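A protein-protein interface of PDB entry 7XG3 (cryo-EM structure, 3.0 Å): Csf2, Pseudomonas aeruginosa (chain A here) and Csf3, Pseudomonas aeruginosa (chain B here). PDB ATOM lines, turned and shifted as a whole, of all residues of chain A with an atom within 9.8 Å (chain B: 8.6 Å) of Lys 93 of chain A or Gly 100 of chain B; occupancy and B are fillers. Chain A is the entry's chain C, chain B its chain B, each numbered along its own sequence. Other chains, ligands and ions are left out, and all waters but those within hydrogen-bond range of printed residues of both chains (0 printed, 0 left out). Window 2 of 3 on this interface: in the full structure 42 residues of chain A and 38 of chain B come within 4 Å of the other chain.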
ATOM      1  N   GLU A  84       5.764  12.879  -8.834  1.00  0.00           N
ATOM      2  CA  GLU A  84       7.200  12.812  -8.550  1.00  0.00           C
ATOM      3  C   GLU A  84       7.604  13.108  -7.106  1.00  0.00           C
ATOM      4  O   GLU A  84       8.477  12.379  -6.606  1.00  0.00           O
ATOM      5  CB  GLU A  84       8.003  13.714  -9.502  1.00  0.00           C
ATOM      6  CG  GLU A  84       9.351  13.150  -9.892  1.00  0.00           C
ATOM      7  CD  GLU A  84      10.497  13.878  -9.197  1.00  0.00           C
ATOM      8  OE1 GLU A  84      11.674  13.616  -9.526  1.00  0.00           O
ATOM      9  OE2 GLU A  84      10.221  14.734  -8.331  1.00  0.00           O
ATOM     10  N   ALA A  86       5.868  12.498  -4.429  1.00  0.00           N
ATOM     11  CA  ALA A  86       5.423  11.314  -3.701  1.00  0.00           C
ATOM     12  C   ALA A  86       6.339  10.125  -3.967  1.00  0.00           C
ATOM     13  O   ALA A  86       6.674   9.367  -3.048  1.00  0.00           O
ATOM     14  CB  ALA A  86       3.981  10.977  -4.078  1.00  0.00           C
ATOM     15  N   LEU A  87       6.772   9.955  -5.218  1.00  0.00           N
ATOM     16  CA  LEU A  87       7.605   8.804  -5.546  1.00  0.00           C
ATOM     17  C   LEU A  87       9.069   8.998  -5.160  1.00  0.00           C
ATOM     18  O   LEU A  87       9.802   8.008  -5.084  1.00  0.00           O
ATOM     19  CB  LEU A  87       7.497   8.471  -7.034  1.00  0.00           C
ATOM     20  CG  LEU A  87       6.125   8.015  -7.541  1.00  0.00           C
ATOM     21  CD1 LEU A  87       6.182   7.641  -9.012  1.00  0.00           C
ATOM     22  CD2 LEU A  87       5.566   6.873  -6.717  1.00  0.00           C
ATOM     23  N   VAL A  88       9.521  10.232  -4.918  1.00  0.00           N
ATOM     24  CA  VAL A  88      10.879  10.426  -4.411  1.00  0.00           C
ATOM     25  C   VAL A  88      10.927  10.607  -2.895  1.00  0.00           C
ATOM     26  O   VAL A  88      12.016  10.506  -2.311  1.00  0.00           O
ATOM     27  CB  VAL A  88      11.604  11.606  -5.094  1.00  0.00           C
ATOM     28  CG1 VAL A  88      11.625  11.428  -6.606  1.00  0.00           C
ATOM     29  CG2 VAL A  88      11.016  12.946  -4.667  1.00  0.00           C
ATOM     30  N   GLU A  89       9.792  10.871  -2.242  1.00  0.00           N
ATOM     31  CA  GLU A  89       9.764  10.801  -0.785  1.00  0.00           C
ATOM     32  C   GLU A  89       9.707   9.365  -0.287  1.00  0.00           C
ATOM     33  O   GLU A  89       9.919   9.125   0.906  1.00  0.00           O
ATOM     34  CB  GLU A  89       8.577  11.589  -0.229  1.00  0.00           C
ATOM     35  CG  GLU A  89       8.791  13.093  -0.161  1.00  0.00           C
ATOM     36  CD  GLU A  89       7.485  13.858  -0.225  1.00  0.00           C
ATOM     37  OE1 GLU A  89       6.442  13.228  -0.500  1.00  0.00           O
ATOM     38  OE2 GLU A  89       7.500  15.088  -0.008  1.00  0.00           O
ATOM     39  N   LYS A  90       9.428   8.411  -1.173  1.00  0.00           N
ATOM     40  CA  LYS A  90       9.408   6.996  -0.835  1.00  0.00           C
ATOM     41  C   LYS A  90      10.680   6.290  -1.296  1.00  0.00           C
ATOM     42  O   LYS A  90      11.147   5.362  -0.625  1.00  0.00           O
ATOM     43  CB  LYS A  90       8.145   6.358  -1.431  1.00  0.00           C
ATOM     44  CG  LYS A  90       8.141   4.851  -1.611  1.00  0.00           C
ATOM     45  CD  LYS A  90       6.746   4.365  -1.962  1.00  0.00           C
ATOM     46  CE  LYS A  90       5.761   4.653  -0.838  1.00  0.00           C
ATOM     47  NZ  LYS A  90       4.459   5.164  -1.349  1.00  0.00           N
ATOM     48  N   GLY A  91      11.298   6.763  -2.376  1.00  0.00           N
ATOM     49  CA  GLY A  91      12.541   6.191  -2.854  1.00  0.00           C
ATOM     50  C   GLY A  91      12.355   5.323  -4.078  1.00  0.00           C
ATOM     51  O   GLY A  91      13.200   4.481  -4.394  1.00  0.00           O
ATOM     52  N   ASN A  92      11.244   5.528  -4.776  1.00  0.00           N
ATOM     53  CA  ASN A  92      10.923   4.726  -5.943  1.00  0.00           C
ATOM     54  C   ASN A  92      11.797   5.112  -7.132  1.00  0.00           C
ATOM     55  O   ASN A  92      12.116   6.281  -7.357  1.00  0.00           O
ATOM     56  CB  ASN A  92       9.449   4.885  -6.300  1.00  0.00           C
ATOM     57  CG  ASN A  92       8.536   4.214  -5.298  1.00  0.00           C
ATOM     58  OD1 ASN A  92       7.353   4.527  -5.220  1.00  0.00           O
ATOM     59  ND2 ASN A  92       9.080   3.277  -4.533  1.00  0.00           N
ATOM     60  N   LYS A  93      12.182   4.096  -7.904  1.00  0.00           N
ATOM     61  CA  LYS A  93      13.029   4.295  -9.078  1.00  0.00           C
ATOM     62  C   LYS A  93      12.309   3.667 -10.266  1.00  0.00           C
ATOM     63  O   LYS A  93      12.183   2.441 -10.341  1.00  0.00           O
ATOM     64  CB  LYS A  93      14.408   3.682  -8.873  1.00  0.00           C
ATOM     65  CG  LYS A  93      15.194   4.287  -7.723  1.00  0.00           C
ATOM     66  CD  LYS A  93      16.530   3.591  -7.545  1.00  0.00           C
ATOM     67  CE  LYS A  93      17.451   4.395  -6.645  1.00  0.00           C
ATOM     68  NZ  LYS A  93      17.711   5.752  -7.198  1.00  0.00           N
ATOM     69  N   LEU A  94      11.841   4.508 -11.183  1.00  0.00           N
ATOM     70  CA  LEU A  94      11.140   4.025 -12.361  1.00  0.00           C
ATOM     71  C   LEU A  94      12.132   3.451 -13.370  1.00  0.00           C
ATOM     72  O   LEU A  94      13.346   3.644 -13.278  1.00  0.00           O
ATOM     73  CB  LEU A  94      10.315   5.144 -12.994  1.00  0.00           C
ATOM     74  CG  LEU A  94       8.888   5.371 -12.488  1.00  0.00           C
ATOM     75  CD1 LEU A  94       8.883   6.107 -11.162  1.00  0.00           C
ATOM     76  CD2 LEU A  94       8.066   6.120 -13.524  1.00  0.00           C
ATOM     77  N   SER A  95      11.597   2.733 -14.350  1.00  0.00           N
ATOM     78  CA  SER A  95      12.390   2.158 -15.423  1.00  0.00           C
ATOM     79  C   SER A  95      11.954   2.771 -16.740  1.00  0.00           C
ATOM     80  O   SER A  95      10.795   3.166 -16.893  1.00  0.00           O
ATOM     81  CB  SER A  95      12.233   0.638 -15.483  1.00  0.00           C
ATOM     82  OG  SER A  95      10.954   0.285 -15.982  1.00  0.00           O
ATOM     83  N   ILE A  96      12.888   2.860 -17.689  1.00  0.00           N
ATOM     84  CA  ILE A  96      12.534   3.327 -19.020  1.00  0.00           C
ATOM     85  C   ILE A  96      11.700   2.262 -19.714  1.00  0.00           C
ATOM     86  O   ILE A  96      12.078   1.085 -19.786  1.00  0.00           O
ATOM     87  CB  ILE A  96      13.800   3.706 -19.806  1.00  0.00           C
ATOM     88  CG1 ILE A  96      14.209   5.132 -19.449  1.00  0.00           C
ATOM     89  CG2 ILE A  96      13.588   3.597 -21.302  1.00  0.00           C
ATOM     90  CD1 ILE A  96      13.181   6.173 -19.833  1.00  0.00           C
ATOM     91  N   ALA A  98       8.585   2.034 -18.331  1.00  0.00           N
ATOM     92  CA  ALA A  98       7.570   2.432 -17.365  1.00  0.00           C
ATOM     93  C   ALA A  98       7.549   3.936 -17.179  1.00  0.00           C
ATOM     94  O   ALA A  98       6.474   4.526 -17.010  1.00  0.00           O
ATOM     95  CB  ALA A  98       7.814   1.740 -16.016  1.00  0.00           C
ATOM     96  N   TYR A  99       8.724   4.570 -17.191  1.00  0.00           N
ATOM     97  CA  TYR A  99       8.794   6.023 -17.244  1.00  0.00           C
ATOM     98  C   TYR A  99       8.288   6.526 -18.585  1.00  0.00           C
ATOM     99  O   TYR A  99       7.649   7.579 -18.662  1.00  0.00           O
ATOM    100  CB  TYR A  99      10.235   6.476 -17.001  1.00  0.00           C
ATOM    101  CG  TYR A  99      10.480   7.975 -17.010  1.00  0.00           C
ATOM    102  CD1 TYR A  99      10.814   8.655 -18.181  1.00  0.00           C
ATOM    103  CD2 TYR A  99      10.435   8.698 -15.828  1.00  0.00           C
ATOM    104  CE1 TYR A  99      11.046  10.017 -18.171  1.00  0.00           C
ATOM    105  CE2 TYR A  99      10.679  10.052 -15.810  1.00  0.00           C
ATOM    106  CZ  TYR A  99      10.977  10.707 -16.981  1.00  0.00           C
ATOM    107  OH  TYR A  99      11.210  12.061 -16.948  1.00  0.00           O
ATOM    108  N   TYR A 103       5.147   8.969 -18.648  1.00  0.00           N
ATOM    109  CA  TYR A 103       5.438  10.338 -19.052  1.00  0.00           C
ATOM    110  C   TYR A 103       5.082  10.606 -20.506  1.00  0.00           C
ATOM    111  O   TYR A 103       4.825  11.755 -20.877  1.00  0.00           O
ATOM    112  CB  TYR A 103       6.915  10.654 -18.810  1.00  0.00           C
ATOM    113  CG  TYR A 103       7.217  11.080 -17.393  1.00  0.00           C
ATOM    114  CD1 TYR A 103       7.118  10.178 -16.339  1.00  0.00           C
ATOM    115  CD2 TYR A 103       7.574  12.391 -17.103  1.00  0.00           C
ATOM    116  CE1 TYR A 103       7.366  10.569 -15.040  1.00  0.00           C
ATOM    117  CE2 TYR A 103       7.832  12.789 -15.805  1.00  0.00           C
ATOM    118  CZ  TYR A 103       7.732  11.871 -14.780  1.00  0.00           C
ATOM    119  OH  TYR A 103       7.984  12.250 -13.484  1.00  0.00           O
ATOM    120  N   LEU A 333       0.846   4.782  -3.301  1.00  0.00           N
ATOM    121  CA  LEU A 333       1.512   4.258  -4.489  1.00  0.00           C
ATOM    122  C   LEU A 333       2.993   4.003  -4.231  1.00  0.00           C
ATOM    123  O   LEU A 333       3.683   4.813  -3.605  1.00  0.00           O
ATOM    124  CB  LEU A 333       1.340   5.220  -5.664  1.00  0.00           C
ATOM    125  CG  LEU A 333      -0.089   5.373  -6.181  1.00  0.00           C
ATOM    126  CD1 LEU A 333      -0.134   6.309  -7.380  1.00  0.00           C
ATOM    127  CD2 LEU A 333      -0.691   4.016  -6.521  1.00  0.00           C
ATOM    128  N   SER A 334       3.480   2.863  -4.725  1.00  0.00           N
ATOM    129  CA  SER A 334       4.854   2.427  -4.503  1.00  0.00           C
ATOM    130  C   SER A 334       5.566   2.044  -5.797  1.00  0.00           C
ATOM    131  O   SER A 334       6.572   1.327  -5.751  1.00  0.00           O
ATOM    132  CB  SER A 334       4.885   1.259  -3.517  1.00  0.00           C
ATOM    133  OG  SER A 334       4.246   0.117  -4.058  1.00  0.00           O
ATOM    134  N   SER A 335       5.019   2.454  -6.948  1.00  0.00           N
ATOM    135  CA  SER A 335       5.611   2.371  -8.288  1.00  0.00           C
ATOM    136  C   SER A 335       5.816   0.953  -8.818  1.00  0.00           C
ATOM    137  O   SER A 335       6.299   0.783  -9.942  1.00  0.00           O
ATOM    138  CB  SER A 335       6.943   3.126  -8.350  1.00  0.00           C
ATOM    139  OG  SER A 335       7.999   2.328  -7.844  1.00  0.00           O
ATOM    140  N   LYS A 336       5.457  -0.071  -8.041  1.00  0.00           N
ATOM    141  CA  LYS A 336       5.402  -1.416  -8.599  1.00  0.00           C
ATOM    142  C   LYS A 336       4.201  -1.566  -9.518  1.00  0.00           C
ATOM    143  O   LYS A 336       4.219  -2.388 -10.441  1.00  0.00           O
ATOM    144  CB  LYS A 336       5.364  -2.454  -7.476  1.00  0.00           C
ATOM    145  CG  LYS A 336       4.237  -2.259  -6.473  1.00  0.00           C
ATOM    146  CD  LYS A 336       3.726  -3.589  -5.947  1.00  0.00           C
ATOM    147  CE  LYS A 336       2.936  -4.337  -7.009  1.00  0.00           C
ATOM    148  NZ  LYS A 336       1.649  -3.659  -7.325  1.00  0.00           N
ATOM    149  N   GLU A 337       3.162  -0.763  -9.288  1.00  0.00           N
ATOM    150  CA  GLU A 337       2.007  -0.743 -10.175  1.00  0.00           C
ATOM    151  C   GLU A 337       2.343  -0.095 -11.513  1.00  0.00           C
ATOM    152  O   GLU A 337       1.802  -0.493 -12.547  1.00  0.00           O
ATOM    153  CB  GLU A 337       0.830  -0.041  -9.488  1.00  0.00           C
ATOM    154  CG  GLU A 337       1.036   1.431  -9.130  1.00  0.00           C
ATOM    155  CD  GLU A 337       1.827   1.642  -7.851  1.00  0.00           C
ATOM    156  OE1 GLU A 337       1.964   0.676  -7.070  1.00  0.00           O
ATOM    157  OE2 GLU A 337       2.328   2.763  -7.637  1.00  0.00           O
ATOM    158  N   PHE A 338       3.264   0.877 -11.521  1.00  0.00           N
ATOM    159  CA  PHE A 338       3.741   1.449 -12.780  1.00  0.00           C
ATOM    160  C   PHE A 338       4.527   0.419 -13.584  1.00  0.00           C
ATOM    161  O   PHE A 338       4.362   0.302 -14.807  1.00  0.00           O
ATOM    162  CB  PHE A 338       4.611   2.677 -12.504  1.00  0.00           C
ATOM    163  CG  PHE A 338       3.840   3.898 -12.096  1.00  0.00           C
ATOM    164  CD1 PHE A 338       3.083   4.597 -13.021  1.00  0.00           C
ATOM    165  CD2 PHE A 338       3.889   4.357 -10.791  1.00  0.00           C
ATOM    166  CE1 PHE A 338       2.376   5.728 -12.646  1.00  0.00           C
ATOM    167  CE2 PHE A 338       3.188   5.485 -10.408  1.00  0.00           C
ATOM    168  CZ  PHE A 338       2.430   6.171 -11.338  1.00  0.00           C
ATOM    169  N   GLU A 339       5.386  -0.342 -12.900  1.00  0.00           N
ATOM    170  CA  GLU A 339       6.172  -1.381 -13.555  1.00  0.00           C
ATOM    171  C   GLU A 339       5.283  -2.512 -14.055  1.00  0.00           C
ATOM    172  O   GLU A 339       5.533  -3.082 -15.124  1.00  0.00           O
ATOM    173  CB  GLU A 339       7.237  -1.899 -12.583  1.00  0.00           C
ATOM    174  CG  GLU A 339       8.174  -2.978 -13.120  1.00  0.00           C
ATOM    175  CD  GLU A 339       7.711  -4.388 -12.790  1.00  0.00           C
ATOM    176  OE1 GLU A 339       6.908  -4.550 -11.847  1.00  0.00           O
ATOM    177  OE2 GLU A 339       8.165  -5.337 -13.463  1.00  0.00           O
ATOM    178  N   GLN A 343       4.952  -3.648 -18.172  1.00  0.00           N
ATOM    179  CA  GLN A 343       5.140  -5.004 -18.666  1.00  0.00           C
ATOM    180  C   GLN A 343       4.034  -5.929 -18.171  1.00  0.00           C
ATOM    181  O   GLN A 343       3.311  -6.527 -18.967  1.00  0.00           O
ATOM    182  CB  GLN A 343       6.508  -5.537 -18.238  1.00  0.00           C
ATOM    183  CG  GLN A 343       7.662  -4.605 -18.564  1.00  0.00           C
ATOM    184  CD  GLN A 343       8.209  -3.906 -17.335  1.00  0.00           C
ATOM    185  OE1 GLN A 343       8.070  -4.397 -16.216  1.00  0.00           O
ATOM    186  NE2 GLN A 343       8.836  -2.754 -17.538  1.00  0.00           N
ATOM    187  N   ALA B  93      13.547  14.007 -18.252  1.00  0.00           N
ATOM    188  CA  ALA B  93      14.224  12.718 -18.160  1.00  0.00           C
ATOM    189  C   ALA B  93      15.642  12.873 -17.627  1.00  0.00           C
ATOM    190  O   ALA B  93      16.099  12.054 -16.826  1.00  0.00           O
ATOM    191  CB  ALA B  93      14.235  12.032 -19.523  1.00  0.00           C
ATOM    192  N   ALA B  94      16.342  13.931 -18.041  1.00  0.00           N
ATOM    193  CA  ALA B  94      17.694  14.176 -17.551  1.00  0.00           C
ATOM    194  C   ALA B  94      17.689  14.543 -16.074  1.00  0.00           C
ATOM    195  O   ALA B  94      18.513  14.043 -15.292  1.00  0.00           O
ATOM    196  CB  ALA B  94      18.357  15.279 -18.376  1.00  0.00           C
ATOM    197  N   ARG B  95      16.751  15.405 -15.663  1.00  0.00           N
ATOM    198  CA  ARG B  95      16.701  15.776 -14.250  1.00  0.00           C
ATOM    199  C   ARG B  95      16.229  14.614 -13.376  1.00  0.00           C
ATOM    200  O   ARG B  95      16.655  14.501 -12.221  1.00  0.00           O
ATOM    201  CB  ARG B  95      15.837  17.027 -14.043  1.00  0.00           C
ATOM    202  CG  ARG B  95      14.338  16.826 -14.078  1.00  0.00           C
ATOM    203  CD  ARG B  95      13.619  17.798 -13.160  1.00  0.00           C
ATOM    204  NE  ARG B  95      13.938  17.563 -11.757  1.00  0.00           N
ATOM    205  CZ  ARG B  95      13.145  17.891 -10.746  1.00  0.00           C
ATOM    206  NH1 ARG B  95      11.962  18.445 -10.949  1.00  0.00           N
ATOM    207  NH2 ARG B  95      13.545  17.647  -9.501  1.00  0.00           N
ATOM    208  N   HIS B  96      15.410  13.708 -13.920  1.00  0.00           N
ATOM    209  CA  HIS B  96      15.011  12.529 -13.159  1.00  0.00           C
ATOM    210  C   HIS B  96      16.127  11.493 -13.124  1.00  0.00           C
ATOM    211  O   HIS B  96      16.240  10.728 -12.158  1.00  0.00           O
ATOM    212  CB  HIS B  96      13.734  11.936 -13.751  1.00  0.00           C
ATOM    213  CG  HIS B  96      12.528  12.803 -13.567  1.00  0.00           C
ATOM    214  ND1 HIS B  96      11.550  12.928 -14.528  1.00  0.00           N
ATOM    215  CD2 HIS B  96      12.163  13.617 -12.551  1.00  0.00           C
ATOM    216  CE1 HIS B  96      10.625  13.769 -14.104  1.00  0.00           C
ATOM    217  NE2 HIS B  96      10.971  14.197 -12.903  1.00  0.00           N
ATOM    218  N   ARG B  97      16.951  11.448 -14.174  1.00  0.00           N
ATOM    219  CA  ARG B  97      18.120  10.577 -14.186  1.00  0.00           C
ATOM    220  C   ARG B  97      19.146  11.011 -13.151  1.00  0.00           C
ATOM    221  O   ARG B  97      19.772  10.163 -12.505  1.00  0.00           O
ATOM    222  CB  ARG B  97      18.733  10.567 -15.587  1.00  0.00           C
ATOM    223  CG  ARG B  97      19.725   9.454 -15.865  1.00  0.00           C
ATOM    224  CD  ARG B  97      19.945   9.319 -17.364  1.00  0.00           C
ATOM    225  NE  ARG B  97      20.934   8.304 -17.705  1.00  0.00           N
ATOM    226  CZ  ARG B  97      22.138   8.566 -18.194  1.00  0.00           C
ATOM    227  NH1 ARG B  97      22.539   9.807 -18.413  1.00  0.00           N
ATOM    228  NH2 ARG B  97      22.957   7.559 -18.478  1.00  0.00           N
ATOM    229  N   GLN B  98      19.331  12.320 -12.975  1.00  0.00           N
ATOM    230  CA  GLN B  98      20.221  12.786 -11.914  1.00  0.00           C
ATOM    231  C   GLN B  98      19.592  12.626 -10.537  1.00  0.00           C
ATOM    232  O   GLN B  98      20.286  12.295  -9.568  1.00  0.00           O
ATOM    233  CB  GLN B  98      20.625  14.237 -12.143  1.00  0.00           C
ATOM    234  CG  GLN B  98      21.215  14.508 -13.490  1.00  0.00           C
ATOM    235  CD  GLN B  98      22.235  13.472 -13.929  1.00  0.00           C
ATOM    236  OE1 GLN B  98      23.371  13.464 -13.455  1.00  0.00           O
ATOM    237  NE2 GLN B  98      21.846  12.616 -14.870  1.00  0.00           N
ATOM    238  N   SER B  99      18.282  12.863 -10.420  1.00  0.00           N
ATOM    239  CA  SER B  99      17.648  12.807  -9.107  1.00  0.00           C
ATOM    240  C   SER B  99      17.486  11.382  -8.595  1.00  0.00           C
ATOM    241  O   SER B  99      17.193  11.192  -7.410  1.00  0.00           O
ATOM    242  CB  SER B  99      16.286  13.499  -9.144  1.00  0.00           C
ATOM    243  OG  SER B  99      15.347  12.735  -9.876  1.00  0.00           O
ATOM    244  N   GLY B 100      17.677  10.379  -9.452  1.00  0.00           N
ATOM    245  CA  GLY B 100      17.540   8.993  -9.079  1.00  0.00           C
ATOM    246  C   GLY B 100      16.158   8.422  -9.300  1.00  0.00           C
ATOM    247  O   GLY B 100      15.968   7.213  -9.131  1.00  0.00           O
ATOM    248  N   TYR B 101      15.189   9.260  -9.677  1.00  0.00           N
ATOM    249  CA  TYR B 101      13.838   8.768  -9.924  1.00  0.00           C
ATOM    250  C   TYR B 101      13.775   8.000 -11.239  1.00  0.00           C
ATOM    251  O   TYR B 101      12.884   7.166 -11.429  1.00  0.00           O
ATOM    252  CB  TYR B 101      12.860   9.956  -9.861  1.00  0.00           C
ATOM    253  CG  TYR B 101      11.461   9.812 -10.455  1.00  0.00           C
ATOM    254  CD1 TYR B 101      11.215   9.955 -11.825  1.00  0.00           C
ATOM    255  CD2 TYR B 101      10.363   9.699  -9.613  1.00  0.00           C
ATOM    256  CE1 TYR B 101       9.930   9.862 -12.333  1.00  0.00           C
ATOM    257  CE2 TYR B 101       9.081   9.603 -10.111  1.00  0.00           C
ATOM    258  CZ  TYR B 101       8.867   9.694 -11.467  1.00  0.00           C
ATOM    259  OH  TYR B 101       7.582   9.610 -11.952  1.00  0.00           O
ATOM    260  N   LEU B 102      14.708   8.262 -12.146  1.00  0.00           N
ATOM    261  CA  LEU B 102      14.811   7.548 -13.407  1.00  0.00           C
ATOM    262  C   LEU B 102      16.073   6.700 -13.410  1.00  0.00           C
ATOM    263  O   LEU B 102      17.147   7.165 -13.018  1.00  0.00           O
ATOM    264  CB  LEU B 102      14.836   8.517 -14.590  1.00  0.00           C
ATOM    265  CG  LEU B 102      14.901   7.901 -15.986  1.00  0.00           C
ATOM    266  CD1 LEU B 102      13.805   6.873 -16.163  1.00  0.00           C
ATOM    267  CD2 LEU B 102      14.817   8.972 -17.053  1.00  0.00           C
ATOM    268  N   GLN B 103      15.936   5.456 -13.853  1.00  0.00           N
ATOM    269  CA  GLN B 103      17.050   4.522 -13.958  1.00  0.00           C
ATOM    270  C   GLN B 103      17.250   4.257 -15.447  1.00  0.00           C
ATOM    271  O   GLN B 103      16.654   3.340 -16.014  1.00  0.00           O
ATOM    272  CB  GLN B 103      16.766   3.244 -13.173  1.00  0.00           C
ATOM    273  CG  GLN B 103      16.961   3.377 -11.664  1.00  0.00           C
ATOM    274  CD  GLN B 103      18.409   3.234 -11.228  1.00  0.00           C
ATOM    275  OE1 GLN B 103      19.254   4.076 -11.534  1.00  0.00           O
ATOM    276  NE2 GLN B 103      18.700   2.159 -10.503  1.00  0.00           N
ATOM    277  N   LEU B 104      18.088   5.076 -16.078  1.00  0.00           N
ATOM    278  CA  LEU B 104      18.338   5.025 -17.515  1.00  0.00           C
ATOM    279  C   LEU B 104      19.831   4.805 -17.725  1.00  0.00           C
ATOM    280  O   LEU B 104      20.641   5.689 -17.422  1.00  0.00           O
ATOM    281  CB  LEU B 104      17.863   6.313 -18.189  1.00  0.00           C
ATOM    282  CG  LEU B 104      17.950   6.529 -19.705  1.00  0.00           C
ATOM    283  CD1 LEU B 104      17.730   5.255 -20.507  1.00  0.00           C
ATOM    284  CD2 LEU B 104      16.969   7.606 -20.134  1.00  0.00           C
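The backbone carbonyl oxygen (O) of Gly 100 of chain B lies within hydrogen-bond range of the side-chain amino group (NZ) of Lys 93 of chain A, 3.0 Å away. NE2 of His 96 of chain B sits close to OE1 of Glu 84 of chain A (3.5 Å). OH of Tyr 99 of chain A is in hydrogen-bond range of ND1 of His 96 of chain B, at 2.6 Å. The side-chain hydroxyl of Tyr 101 of chain B lies within hydrogen-bond range of the side-chain hydroxyl of Tyr 103 of chain A (3.1 Å). N of Ala 93 of chain B is in hydrogen-bond range of OH of Tyr 99 of chain A (3.3 Å). N of Gln 103 of chain B is in hydrogen-bond range of O of Leu 94 of chain A. The backbone carbonyl oxygen (O) of Tyr 101 of chain B sits at hydrogen-bond distance from the backbone NH (N) of Leu 94 of chain A.
Hydrophobic or aromatic side chains of chain B that line the printed part of chain A: Ala 93, His 96, Tyr 101, Leu 102 and Leu 104. Of the 23 printed residues of chain A, 9 touch a printed residue of chain B. Printed residues of chain A that touch a printed residue of chain B: Glu 84, Leu 87, Val 88, Asn 92, Lys 93, Leu 94, Ile 96, Tyr 99 and Tyr 103. Hydrophobic or aromatic side chains of chain A that line the printed part of chain B: Leu 87, Val 88, Leu 94, Ile 96, Tyr 99 and Tyr 103. Among the printed residues, 19 pairs touch across the chains.
OD1 of Asn 92 of chain A sits close to OG of Ser 335 of chain A (3.5 Å). N of Tyr 101 of chain B lies within hydrogen-bond range of O of His 96 of chain B (3.1 Å). The side-chain hydroxyl (OG) of Ser 99 of chain B lies close to the backbone NH (N) of Tyr 101 of chain B (3.5 Å). OD1 of Asn 92 of chain A lies close to O of Ser 334 of chain A (3.3 Å). OG of Ser 99 of chain B lies within hydrogen-bond range of O of His 96 of chain B, at 3.2 Å. NE of Arg 97 of chain B sits at hydrogen-bond distance from O of Leu 104 of chain B (2.6 Å).
Lys 93 of chain A touches just these residues of chain B: Gly 100 (3.0 Å), Tyr 101 (3.7 Å) and Gln 103 (3.8 Å). Printed residues of chain B within 4 Å of Leu 87 of chain A: Tyr 101. Of the printed residues of chain A, Tyr 101 of chain B touches Glu 84, Leu 87, Val 88, Asn 92, Lys 93, Leu 94, Tyr 99 and Tyr 103. Printed residues of chain A within 4 Å of Leu 104 of chain B: Ile 96 (3.7 Å). Printed residues of chain A within 4 Å of Gln 103 of chain B: Lys 93 (3.8 Å) and Leu 94 (3.2 Å). Printed residues of chain B within 4 Å of Ile 96 of chain A: Leu 102 and Leu 104. Ala 86 of chain A touches none of the printed residues of chain B. Gly 91 of chain A touches none of the printed residues of chain B. The nearest residue of chain B that does not touch Lys 93 of chain A is Leu 102 of chain B (5.3 Å). The nearest printed residue of chain A that does not touch Leu 104 of chain B is Leu 94 of chain A (5.7 Å).
Glu 84 of chain A touches Ser 99 of chain B (OE1 to OG, 3.8 Å). CG of Glu 84 of chain A touches CE2 of Tyr 101 of chain B, 3.6 Å away. Tyr 101 of chain B touches Val 88 of chain A. O of Tyr 101 of chain B touches CA of Lys 93 of chain A, 3.7 Å away. CB of Lys 93 of chain A touches CG of Gln 103 of chain B (3.8 Å). CG1 of Ile 96 of chain A touches CD1 of Leu 102 of chain B, 3.7 Å away. Leu 104 of chain B touches Ile 96 of chain A. CE1 of Tyr 101 of chain B touches CE2 of Tyr 99 of chain A, 3.6 Å away. CD1 of Leu 102 of chain B touches CG of Tyr 99 of chain A, 3.6 Å away. His 96 of chain B touches Tyr 103 of chain A.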
